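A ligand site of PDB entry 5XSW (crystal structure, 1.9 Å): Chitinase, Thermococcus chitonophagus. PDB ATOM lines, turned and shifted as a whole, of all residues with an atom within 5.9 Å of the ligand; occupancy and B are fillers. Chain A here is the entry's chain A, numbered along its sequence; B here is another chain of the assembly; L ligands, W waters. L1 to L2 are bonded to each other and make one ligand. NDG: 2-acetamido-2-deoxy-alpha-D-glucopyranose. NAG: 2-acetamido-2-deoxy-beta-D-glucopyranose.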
ATOM      1  N   PRO A 172     -13.328  11.020   7.577  1.00  0.00           N
ATOM      2  CA  PRO A 172     -14.352  10.939   6.507  1.00  0.00           C
ATOM      3  C   PRO A 172     -14.213  12.052   5.441  1.00  0.00           C
ATOM      4  O   PRO A 172     -14.881  13.104   5.518  1.00  0.00           O
ATOM      5  CB  PRO A 172     -15.673  11.061   7.278  1.00  0.00           C
ATOM      6  CG  PRO A 172     -15.308  11.921   8.519  1.00  0.00           C
ATOM      7  CD  PRO A 172     -13.882  11.462   8.884  1.00  0.00           C
ATOM      8  N   LEU A 173     -13.382  11.800   4.439  1.00  0.00           N
ATOM      9  CA  LEU A 173     -12.978  12.854   3.528  1.00  0.00           C
ATOM     10  C   LEU A 173     -14.129  13.082   2.576  1.00  0.00           C
ATOM     11  O   LEU A 173     -14.537  12.144   1.859  1.00  0.00           O
ATOM     12  CB  LEU A 173     -11.722  12.440   2.724  1.00  0.00           C
ATOM     13  CG  LEU A 173     -11.405  13.255   1.461  1.00  0.00           C
ATOM     14  CD1 LEU A 173     -11.126  14.743   1.814  1.00  0.00           C
ATOM     15  CD2 LEU A 173     -10.140  12.604   0.826  1.00  0.00           C
ATOM     16  N   ASN A 174     -14.626  14.321   2.514  1.00  0.00           N
ATOM     17  CA  ASN A 174     -15.716  14.655   1.603  1.00  0.00           C
ATOM     18  C   ASN A 174     -16.891  13.699   1.716  1.00  0.00           C
ATOM     19  O   ASN A 174     -17.529  13.398   0.704  1.00  0.00           O
ATOM     20  CB  ASN A 174     -15.204  14.695   0.157  1.00  0.00           C
ATOM     21  CG  ASN A 174     -14.307  15.897  -0.070  1.00  0.00           C
ATOM     22  OD1 ASN A 174     -14.401  16.854   0.696  1.00  0.00           O
ATOM     23  ND2 ASN A 174     -13.402  15.842  -1.078  1.00  0.00           N
ATOM     24  N   LEU A 175     -17.106  13.220   2.942  1.00  0.00           N
ATOM     25  CA  LEU A 175     -18.190  12.309   3.357  1.00  0.00           C
ATOM     26  C   LEU A 175     -17.991  10.859   2.880  1.00  0.00           C
ATOM     27  O   LEU A 175     -18.900  10.023   3.002  1.00  0.00           O
ATOM     28  CB  LEU A 175     -19.551  12.798   2.874  1.00  0.00           C
ATOM     29  CG  LEU A 175     -19.999  14.193   3.344  1.00  0.00           C
ATOM     30  CD1 LEU A 175     -21.446  14.424   2.901  1.00  0.00           C
ATOM     31  CD2 LEU A 175     -19.856  14.334   4.823  1.00  0.00           C
ATOM     32  N   LYS A 212      -9.196  17.565  -0.349  1.00  0.00           N
ATOM     33  CA  LYS A 212     -10.408  18.237   0.173  1.00  0.00           C
ATOM     34  C   LYS A 212     -11.097  19.012  -0.943  1.00  0.00           C
ATOM     35  O   LYS A 212     -12.340  18.900  -1.127  1.00  0.00           O
ATOM     36  CB  LYS A 212     -10.048  19.167   1.356  1.00  0.00           C
ATOM     37  CG  LYS A 212     -11.231  20.047   1.817  1.00  0.00           C
ATOM     38  CD  LYS A 212     -12.420  19.155   2.265  1.00  0.00           C
ATOM     39  CE  LYS A 212     -13.741  19.877   2.027  1.00  0.00           C
ATOM     40  NZ  LYS A 212     -14.944  19.073   2.311  1.00  0.00           N
ATOM     41  N   GLU A 213     -10.338  19.784  -1.700  1.00  0.00           N
ATOM     42  CA  GLU A 213     -10.936  20.709  -2.703  1.00  0.00           C
ATOM     43  C   GLU A 213     -11.589  19.995  -3.862  1.00  0.00           C
ATOM     44  O   GLU A 213     -12.646  20.451  -4.348  1.00  0.00           O
ATOM     45  CB  GLU A 213      -9.874  21.649  -3.275  1.00  0.00           C
ATOM     46  CG  GLU A 213      -9.422  22.712  -2.225  1.00  0.00           C
ATOM     47  CD  GLU A 213     -10.492  23.748  -1.911  1.00  0.00           C
ATOM     48  OE1 GLU A 213     -10.182  24.600  -1.037  1.00  0.00           O
ATOM     49  OE2 GLU A 213     -11.578  23.759  -2.585  1.00  0.00           O
ATOM     50  N   ASN A 214     -10.970  18.918  -4.355  1.00  0.00           N
ATOM     51  CA  ASN A 214     -11.531  18.241  -5.542  1.00  0.00           C
ATOM     52  C   ASN A 214     -10.995  16.830  -5.738  1.00  0.00           C
ATOM     53  O   ASN A 214     -10.816  16.393  -6.874  1.00  0.00           O
ATOM     54  CB  ASN A 214     -11.230  19.124  -6.785  1.00  0.00           C
ATOM     55  CG  ASN A 214     -11.990  18.710  -8.075  1.00  0.00           C
ATOM     56  OD1 ASN A 214     -12.994  17.998  -8.044  1.00  0.00           O
ATOM     57  ND2 ASN A 214     -11.463  19.182  -9.221  1.00  0.00           N
ATOM     58  N   TRP A 215     -10.722  16.148  -4.633  1.00  0.00           N
ATOM     59  CA  TRP A 215     -10.282  14.757  -4.717  1.00  0.00           C
ATOM     60  C   TRP A 215      -9.062  14.653  -5.648  1.00  0.00           C
ATOM     61  O   TRP A 215      -8.906  13.656  -6.332  1.00  0.00           O
ATOM     62  CB  TRP A 215     -11.430  13.846  -5.247  1.00  0.00           C
ATOM     63  CG  TRP A 215     -12.458  13.460  -4.238  1.00  0.00           C
ATOM     64  CD1 TRP A 215     -13.700  14.083  -4.019  1.00  0.00           C
ATOM     65  CD2 TRP A 215     -12.357  12.403  -3.244  1.00  0.00           C
ATOM     66  NE1 TRP A 215     -14.380  13.399  -3.036  1.00  0.00           N
ATOM     67  CE2 TRP A 215     -13.585  12.393  -2.534  1.00  0.00           C
ATOM     68  CE3 TRP A 215     -11.379  11.449  -2.936  1.00  0.00           C
ATOM     69  CZ2 TRP A 215     -13.856  11.457  -1.515  1.00  0.00           C
ATOM     70  CZ3 TRP A 215     -11.660  10.504  -1.912  1.00  0.00           C
ATOM     71  CH2 TRP A 215     -12.881  10.543  -1.188  1.00  0.00           C
ATOM     72  N   PHE A 225     -19.070   6.573  -4.298  1.00  0.00           N
ATOM     73  CA  PHE A 225     -18.298   7.625  -4.929  1.00  0.00           C
ATOM     74  C   PHE A 225     -17.802   7.307  -6.293  1.00  0.00           C
ATOM     75  O   PHE A 225     -16.593   7.162  -6.479  1.00  0.00           O
ATOM     76  CB  PHE A 225     -17.121   7.982  -4.046  1.00  0.00           C
ATOM     77  CG  PHE A 225     -17.507   8.800  -2.915  1.00  0.00           C
ATOM     78  CD1 PHE A 225     -18.124   8.222  -1.827  1.00  0.00           C
ATOM     79  CD2 PHE A 225     -17.345  10.158  -2.956  1.00  0.00           C
ATOM     80  CE1 PHE A 225     -18.547   8.983  -0.786  1.00  0.00           C
ATOM     81  CE2 PHE A 225     -17.749  10.912  -1.906  1.00  0.00           C
ATOM     82  CZ  PHE A 225     -18.345  10.350  -0.828  1.00  0.00           C
ATOM     83  N   PRO A 240     -12.676  10.331  -7.376  1.00  0.00           N
ATOM     84  CA  PRO A 240     -13.869  11.189  -7.548  1.00  0.00           C
ATOM     85  C   PRO A 240     -13.530  12.631  -7.902  1.00  0.00           C
ATOM     86  O   PRO A 240     -14.259  13.551  -7.532  1.00  0.00           O
ATOM     87  CB  PRO A 240     -14.565  11.123  -6.149  1.00  0.00           C
ATOM     88  CG  PRO A 240     -13.856   9.923  -5.384  1.00  0.00           C
ATOM     89  CD  PRO A 240     -12.406   9.994  -5.954  1.00  0.00           C
ATOM     90  N   GLN A 242     -13.295  15.998 -10.152  1.00  0.00           N
ATOM     91  CA  GLN A 242     -13.904  16.595 -11.371  1.00  0.00           C
ATOM     92  C   GLN A 242     -12.744  17.095 -12.180  1.00  0.00           C
ATOM     93  O   GLN A 242     -12.261  18.232 -11.977  1.00  0.00           O
ATOM     94  CB  GLN A 242     -14.900  17.747 -11.037  1.00  0.00           C
ATOM     95  CG  GLN A 242     -16.062  17.229 -10.201  1.00  0.00           C
ATOM     96  CD  GLN A 242     -17.003  18.333  -9.650  1.00  0.00           C
ATOM     97  OE1 GLN A 242     -17.054  19.451 -10.166  1.00  0.00           O
ATOM     98  NE2 GLN A 242     -17.723  17.990  -8.614  1.00  0.00           N
ATOM     99  N   HIS A 245     -12.600  20.461 -14.262  1.00  0.00           N
ATOM    100  CA  HIS A 245     -13.005  21.726 -13.615  1.00  0.00           C
ATOM    101  C   HIS A 245     -11.982  22.830 -13.924  1.00  0.00           C
ATOM    102  O   HIS A 245     -10.785  22.635 -13.758  1.00  0.00           O
ATOM    103  CB  HIS A 245     -13.143  21.516 -12.114  1.00  0.00           C
ATOM    104  CG  HIS A 245     -13.974  22.564 -11.449  1.00  0.00           C
ATOM    105  ND1 HIS A 245     -13.579  23.883 -11.409  1.00  0.00           N
ATOM    106  CD2 HIS A 245     -15.197  22.508 -10.843  1.00  0.00           C
ATOM    107  CE1 HIS A 245     -14.497  24.600 -10.747  1.00  0.00           C
ATOM    108  NE2 HIS A 245     -15.485  23.787 -10.409  1.00  0.00           N
ATOM    109  N   GLN A 251      -8.794  24.140  -6.758  1.00  0.00           N
ATOM    110  CA  GLN A 251      -9.985  25.050  -6.802  1.00  0.00           C
ATOM    111  C   GLN A 251      -9.586  26.465  -6.579  1.00  0.00           C
ATOM    112  O   GLN A 251     -10.179  27.206  -5.782  1.00  0.00           O
ATOM    113  CB  GLN A 251     -11.062  24.611  -5.783  1.00  0.00           C
ATOM    114  CG  GLN A 251     -11.576  23.167  -6.131  1.00  0.00           C
ATOM    115  CD  GLN A 251     -12.612  23.232  -7.308  1.00  0.00           C
ATOM    116  OE1 GLN A 251     -13.747  23.683  -7.088  1.00  0.00           O
ATOM    117  NE2 GLN A 251     -12.212  22.873  -8.538  1.00  0.00           N
ATOM    118  N   ASN A 337      -9.698  28.926   2.091  1.00  0.00           N
ATOM    119  CA  ASN A 337     -11.096  28.601   1.759  1.00  0.00           C
ATOM    120  C   ASN A 337     -12.071  29.808   1.908  1.00  0.00           C
ATOM    121  O   ASN A 337     -12.931  30.020   1.054  1.00  0.00           O
ATOM    122  CB  ASN A 337     -11.565  27.474   2.654  1.00  0.00           C
ATOM    123  CG  ASN A 337     -13.044  27.092   2.421  1.00  0.00           C
ATOM    124  OD1 ASN A 337     -13.835  27.112   3.345  1.00  0.00           O
ATOM    125  ND2 ASN A 337     -13.406  26.739   1.157  1.00  0.00           N
ATOM    126  N   PHE A 371     -16.015  25.988   4.852  1.00  0.00           N
ATOM    127  CA  PHE A 371     -17.104  25.137   4.320  1.00  0.00           C
ATOM    128  C   PHE A 371     -16.729  23.674   4.207  1.00  0.00           C
ATOM    129  O   PHE A 371     -15.617  23.361   3.805  1.00  0.00           O
ATOM    130  CB  PHE A 371     -17.536  25.634   2.925  1.00  0.00           C
ATOM    131  CG  PHE A 371     -18.210  26.997   2.956  1.00  0.00           C
ATOM    132  CD1 PHE A 371     -19.367  27.189   3.683  1.00  0.00           C
ATOM    133  CD2 PHE A 371     -17.674  28.071   2.270  1.00  0.00           C
ATOM    134  CE1 PHE A 371     -19.989  28.438   3.736  1.00  0.00           C
ATOM    135  CE2 PHE A 371     -18.284  29.322   2.311  1.00  0.00           C
ATOM    136  CZ  PHE A 371     -19.453  29.490   3.055  1.00  0.00           C
ATOM    137  N   GLY A 372     -17.671  22.786   4.534  1.00  0.00           N
ATOM    138  CA  GLY A 372     -17.484  21.346   4.307  1.00  0.00           C
ATOM    139  C   GLY A 372     -16.390  20.774   5.179  1.00  0.00           C
ATOM    140  O   GLY A 372     -15.667  19.865   4.774  1.00  0.00           O
ATOM    141  N   GLY A 373     -16.220  21.315   6.390  1.00  0.00           N
ATOM    142  CA  GLY A 373     -15.205  20.783   7.322  1.00  0.00           C
ATOM    143  C   GLY A 373     -13.790  20.943   6.764  1.00  0.00           C
ATOM    144  O   GLY A 373     -12.898  20.142   7.064  1.00  0.00           O
ATOM    145  N   HIS A 374     -13.580  22.041   6.020  1.00  0.00           N
ATOM    146  CA  HIS A 374     -12.346  22.254   5.275  1.00  0.00           C
ATOM    147  C   HIS A 374     -11.107  22.198   6.192  1.00  0.00           C
ATOM    148  O   HIS A 374     -10.166  21.450   5.923  1.00  0.00           O
ATOM    149  CB  HIS A 374     -12.383  23.628   4.553  1.00  0.00           C
ATOM    150  CG  HIS A 374     -11.365  23.772   3.466  1.00  0.00           C
ATOM    151  ND1 HIS A 374     -10.015  23.980   3.730  1.00  0.00           N
ATOM    152  CD2 HIS A 374     -11.489  23.790   2.106  1.00  0.00           C
ATOM    153  CE1 HIS A 374      -9.365  24.153   2.588  1.00  0.00           C
ATOM    154  NE2 HIS A 374     -10.233  24.017   1.587  1.00  0.00           N
ATOM    155  N   ARG B 338     -20.163  30.880  -6.335  1.00  0.00           N
ATOM    156  CA  ARG B 338     -19.198  29.814  -6.614  1.00  0.00           C
ATOM    157  C   ARG B 338     -18.155  30.167  -7.646  1.00  0.00           C
ATOM    158  O   ARG B 338     -17.192  29.399  -7.843  1.00  0.00           O
ATOM    159  CB  ARG B 338     -19.909  28.524  -7.040  1.00  0.00           C
ATOM    160  CG  ARG B 338     -20.881  27.904  -5.999  1.00  0.00           C
ATOM    161  CD  ARG B 338     -20.254  27.539  -4.681  1.00  0.00           C
ATOM    162  NE  ARG B 338     -19.023  26.781  -4.765  1.00  0.00           N
ATOM    163  CZ  ARG B 338     -18.896  25.485  -5.041  1.00  0.00           C
ATOM    164  NH1 ARG B 338     -19.951  24.737  -5.314  1.00  0.00           N
ATOM    165  NH2 ARG B 338     -17.667  24.943  -5.016  1.00  0.00           N
ATOM    166  N   PHE B 371     -23.470  27.523  -1.939  1.00  0.00           N
ATOM    167  CA  PHE B 371     -23.400  27.146  -0.518  1.00  0.00           C
ATOM    168  C   PHE B 371     -24.569  27.732   0.251  1.00  0.00           C
ATOM    169  O   PHE B 371     -24.946  28.862  -0.002  1.00  0.00           O
ATOM    170  CB  PHE B 371     -22.087  27.629   0.115  1.00  0.00           C
ATOM    171  CG  PHE B 371     -20.829  26.927  -0.440  1.00  0.00           C
ATOM    172  CD1 PHE B 371     -20.662  25.561  -0.288  1.00  0.00           C
ATOM    173  CD2 PHE B 371     -19.815  27.654  -1.041  1.00  0.00           C
ATOM    174  CE1 PHE B 371     -19.514  24.911  -0.787  1.00  0.00           C
ATOM    175  CE2 PHE B 371     -18.676  27.005  -1.555  1.00  0.00           C
ATOM    176  CZ  PHE B 371     -18.548  25.624  -1.410  1.00  0.00           C
HETATM  177  C1  NDG L   1     -18.091  16.816  -0.999  1.00  0.00           C
HETATM  178  C2  NDG L   1     -17.693  17.918  -0.015  1.00  0.00           C
HETATM  179  C3  NDG L   1     -17.358  19.201  -0.695  1.00  0.00           C
HETATM  180  C4  NDG L   1     -16.400  19.073  -1.869  1.00  0.00           C
HETATM  181  C5  NDG L   1     -16.891  17.992  -2.833  1.00  0.00           C
HETATM  182  C6  NDG L   1     -15.821  17.612  -3.849  1.00  0.00           C
HETATM  183  C7  NDG L   1     -18.652  17.810   2.286  1.00  0.00           C
HETATM  184  C8  NDG L   1     -19.819  18.085   3.308  1.00  0.00           C
HETATM  185  O5  NDG L   1     -17.148  16.748  -2.146  1.00  0.00           O
HETATM  186  O3  NDG L   1     -16.783  20.068   0.314  1.00  0.00           O
HETATM  187  O4  NDG L   1     -16.487  20.240  -2.677  1.00  0.00           O
HETATM  188  O6  NDG L   1     -16.358  16.723  -4.833  1.00  0.00           O
HETATM  189  O7  NDG L   1     -17.572  17.389   2.657  1.00  0.00           O
HETATM  190  N2  NDG L   1     -18.804  18.115   0.897  1.00  0.00           N
HETATM  191  O1  NDG L   1     -19.305  17.113  -1.550  1.00  0.00           O
HETATM  192  C1  NAG L   2     -15.463  21.214  -2.555  1.00  0.00           C
HETATM  193  C2  NAG L   2     -15.504  22.122  -3.730  1.00  0.00           C
HETATM  194  C3  NAG L   2     -14.610  23.323  -3.528  1.00  0.00           C
HETATM  195  C4  NAG L   2     -14.870  24.032  -2.236  1.00  0.00           C
HETATM  196  C5  NAG L   2     -14.757  23.064  -1.131  1.00  0.00           C
HETATM  197  C6  NAG L   2     -15.097  23.761   0.158  1.00  0.00           C
HETATM  198  C7  NAG L   2     -15.871  21.313  -6.104  1.00  0.00           C
HETATM  199  C8  NAG L   2     -15.324  20.527  -7.326  1.00  0.00           C
HETATM  200  N2  NAG L   2     -15.092  21.362  -4.930  1.00  0.00           N
HETATM  201  O3  NAG L   2     -14.726  24.274  -4.606  1.00  0.00           O
HETATM  202  O4  NAG L   2     -13.834  24.999  -1.963  1.00  0.00           O
HETATM  203  O5  NAG L   2     -15.708  21.950  -1.309  1.00  0.00           O
HETATM  204  O6  NAG L   2     -15.070  22.692   1.098  1.00  0.00           O
HETATM  205  O7  NAG L   2     -16.945  21.917  -6.103  1.00  0.00           O
HETATM  206  O   HOH W   1     -19.045  16.987  -5.615  1.00  0.00           O
HETATM  207  O   HOH W   2     -18.314  21.367  -8.534  1.00  0.00           O
HETATM  208  O   HOH W   3     -21.326  19.050   0.115  1.00  0.00           O
HETATM  209  O   HOH W   4     -14.177  27.158  -4.607  1.00  0.00           O
HETATM  210  O   HOH W   5     -14.442  16.268  -6.629  1.00  0.00           O
HETATM  211  O   HOH W   6     -17.155  14.258  -3.628  1.00  0.00           O
HETATM  212  O   HOH W   7     -16.911  16.777   5.156  1.00  0.00           O
HETATM  213  O   HOH W   8     -19.528  14.018  -2.235  1.00  0.00           O
HETATM  214  O   HOH W   9     -20.658  15.895  -3.564  1.00  0.00           O
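Water W7 bridges O7 of NDG L1 (2.7 Å) and O of Gly 372 (3.4 Å).
Water W5 lies within hydrogen-bond range of the side-chain amide oxygen of Asn 214 (2.7 Å), an oxygen (O6) of NDG L1 (2.7 Å) and the backbone carbonyl oxygen of Pro 240 (2.9 Å).
Water W1 lies within hydrogen-bond range of an oxygen (O6) of NDG L1 (2.8 Å) and the side-chain amide nitrogen of Gln 242 (3.4 Å).
Water W2 lies within hydrogen-bond range of OE1 of Gln 242 (2.8 Å) and O7 of NAG L2 (2.8 Å).
Water W6 bridges O6 of NDG L1 (2.9 Å) and NE1 of Trp 215 (3.0 Å).
Merely in contact with the ligand: Asn 174 (3.5 Å), Leu 175 (3.9 Å), Asn 214 (3.5 Å), Trp 215 (3.8 Å), Gln 242 (3.5 Å), Asn 337 (3.6 Å), Gly 372 (3.8 Å) and His 374 (3.9 Å).
Hydrophobic or aromatic side chains that line the ligand: Leu 175, Trp 215 and His 374.
The backbone carbonyl oxygen (O) of Glu 213 lies within hydrogen-bond range of a nitrogen (N2) of NAG L2 (2.7 Å).
O4 of NAG L2 lies within hydrogen-bond range of OE2 of Glu 213.
O3 of NAG L2 is in hydrogen-bond range of OE1 of Gln 251 (2.7 Å).
The backbone carbonyl oxygen (O) of Phe 371 of chain A is in hydrogen-bond range of an oxygen (O6) of NAG L2, at 2.8 Å.
The side-chain amino group of Lys 212 sits at hydrogen-bond distance from an oxygen (O3) of NDG L1 (2.9 Å).
NH2 of Arg 338 of chain B lies within hydrogen-bond range of O3 of NAG L2 (3.0 Å).
A ring nitrogen (NE2) of His 374 is in hydrogen-bond range of the side-chain carboxylate (OE1) of Glu 213 (2.7 Å).
The side-chain amide nitrogen (NE2) of Gln 251 sits at hydrogen-bond distance from a ring nitrogen (ND1) of His 245.
OD1 of Asn 337 lies within hydrogen-bond range of N of Phe 371 of chain A (2.9 Å).
The side-chain amino group of Lys 212 sits at hydrogen-bond distance from the side-chain amide oxygen of Asn 174, at 2.8 Å.
NZ of Lys 212 sits at hydrogen-bond distance from O of Gly 372, at 2.7 Å.
NE1 of Trp 215 lies close to ND2 of Asn 174 (3.3 Å).
N of Gln 242 lies within hydrogen-bond range of OD1 of Asn 214 (2.9 Å).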
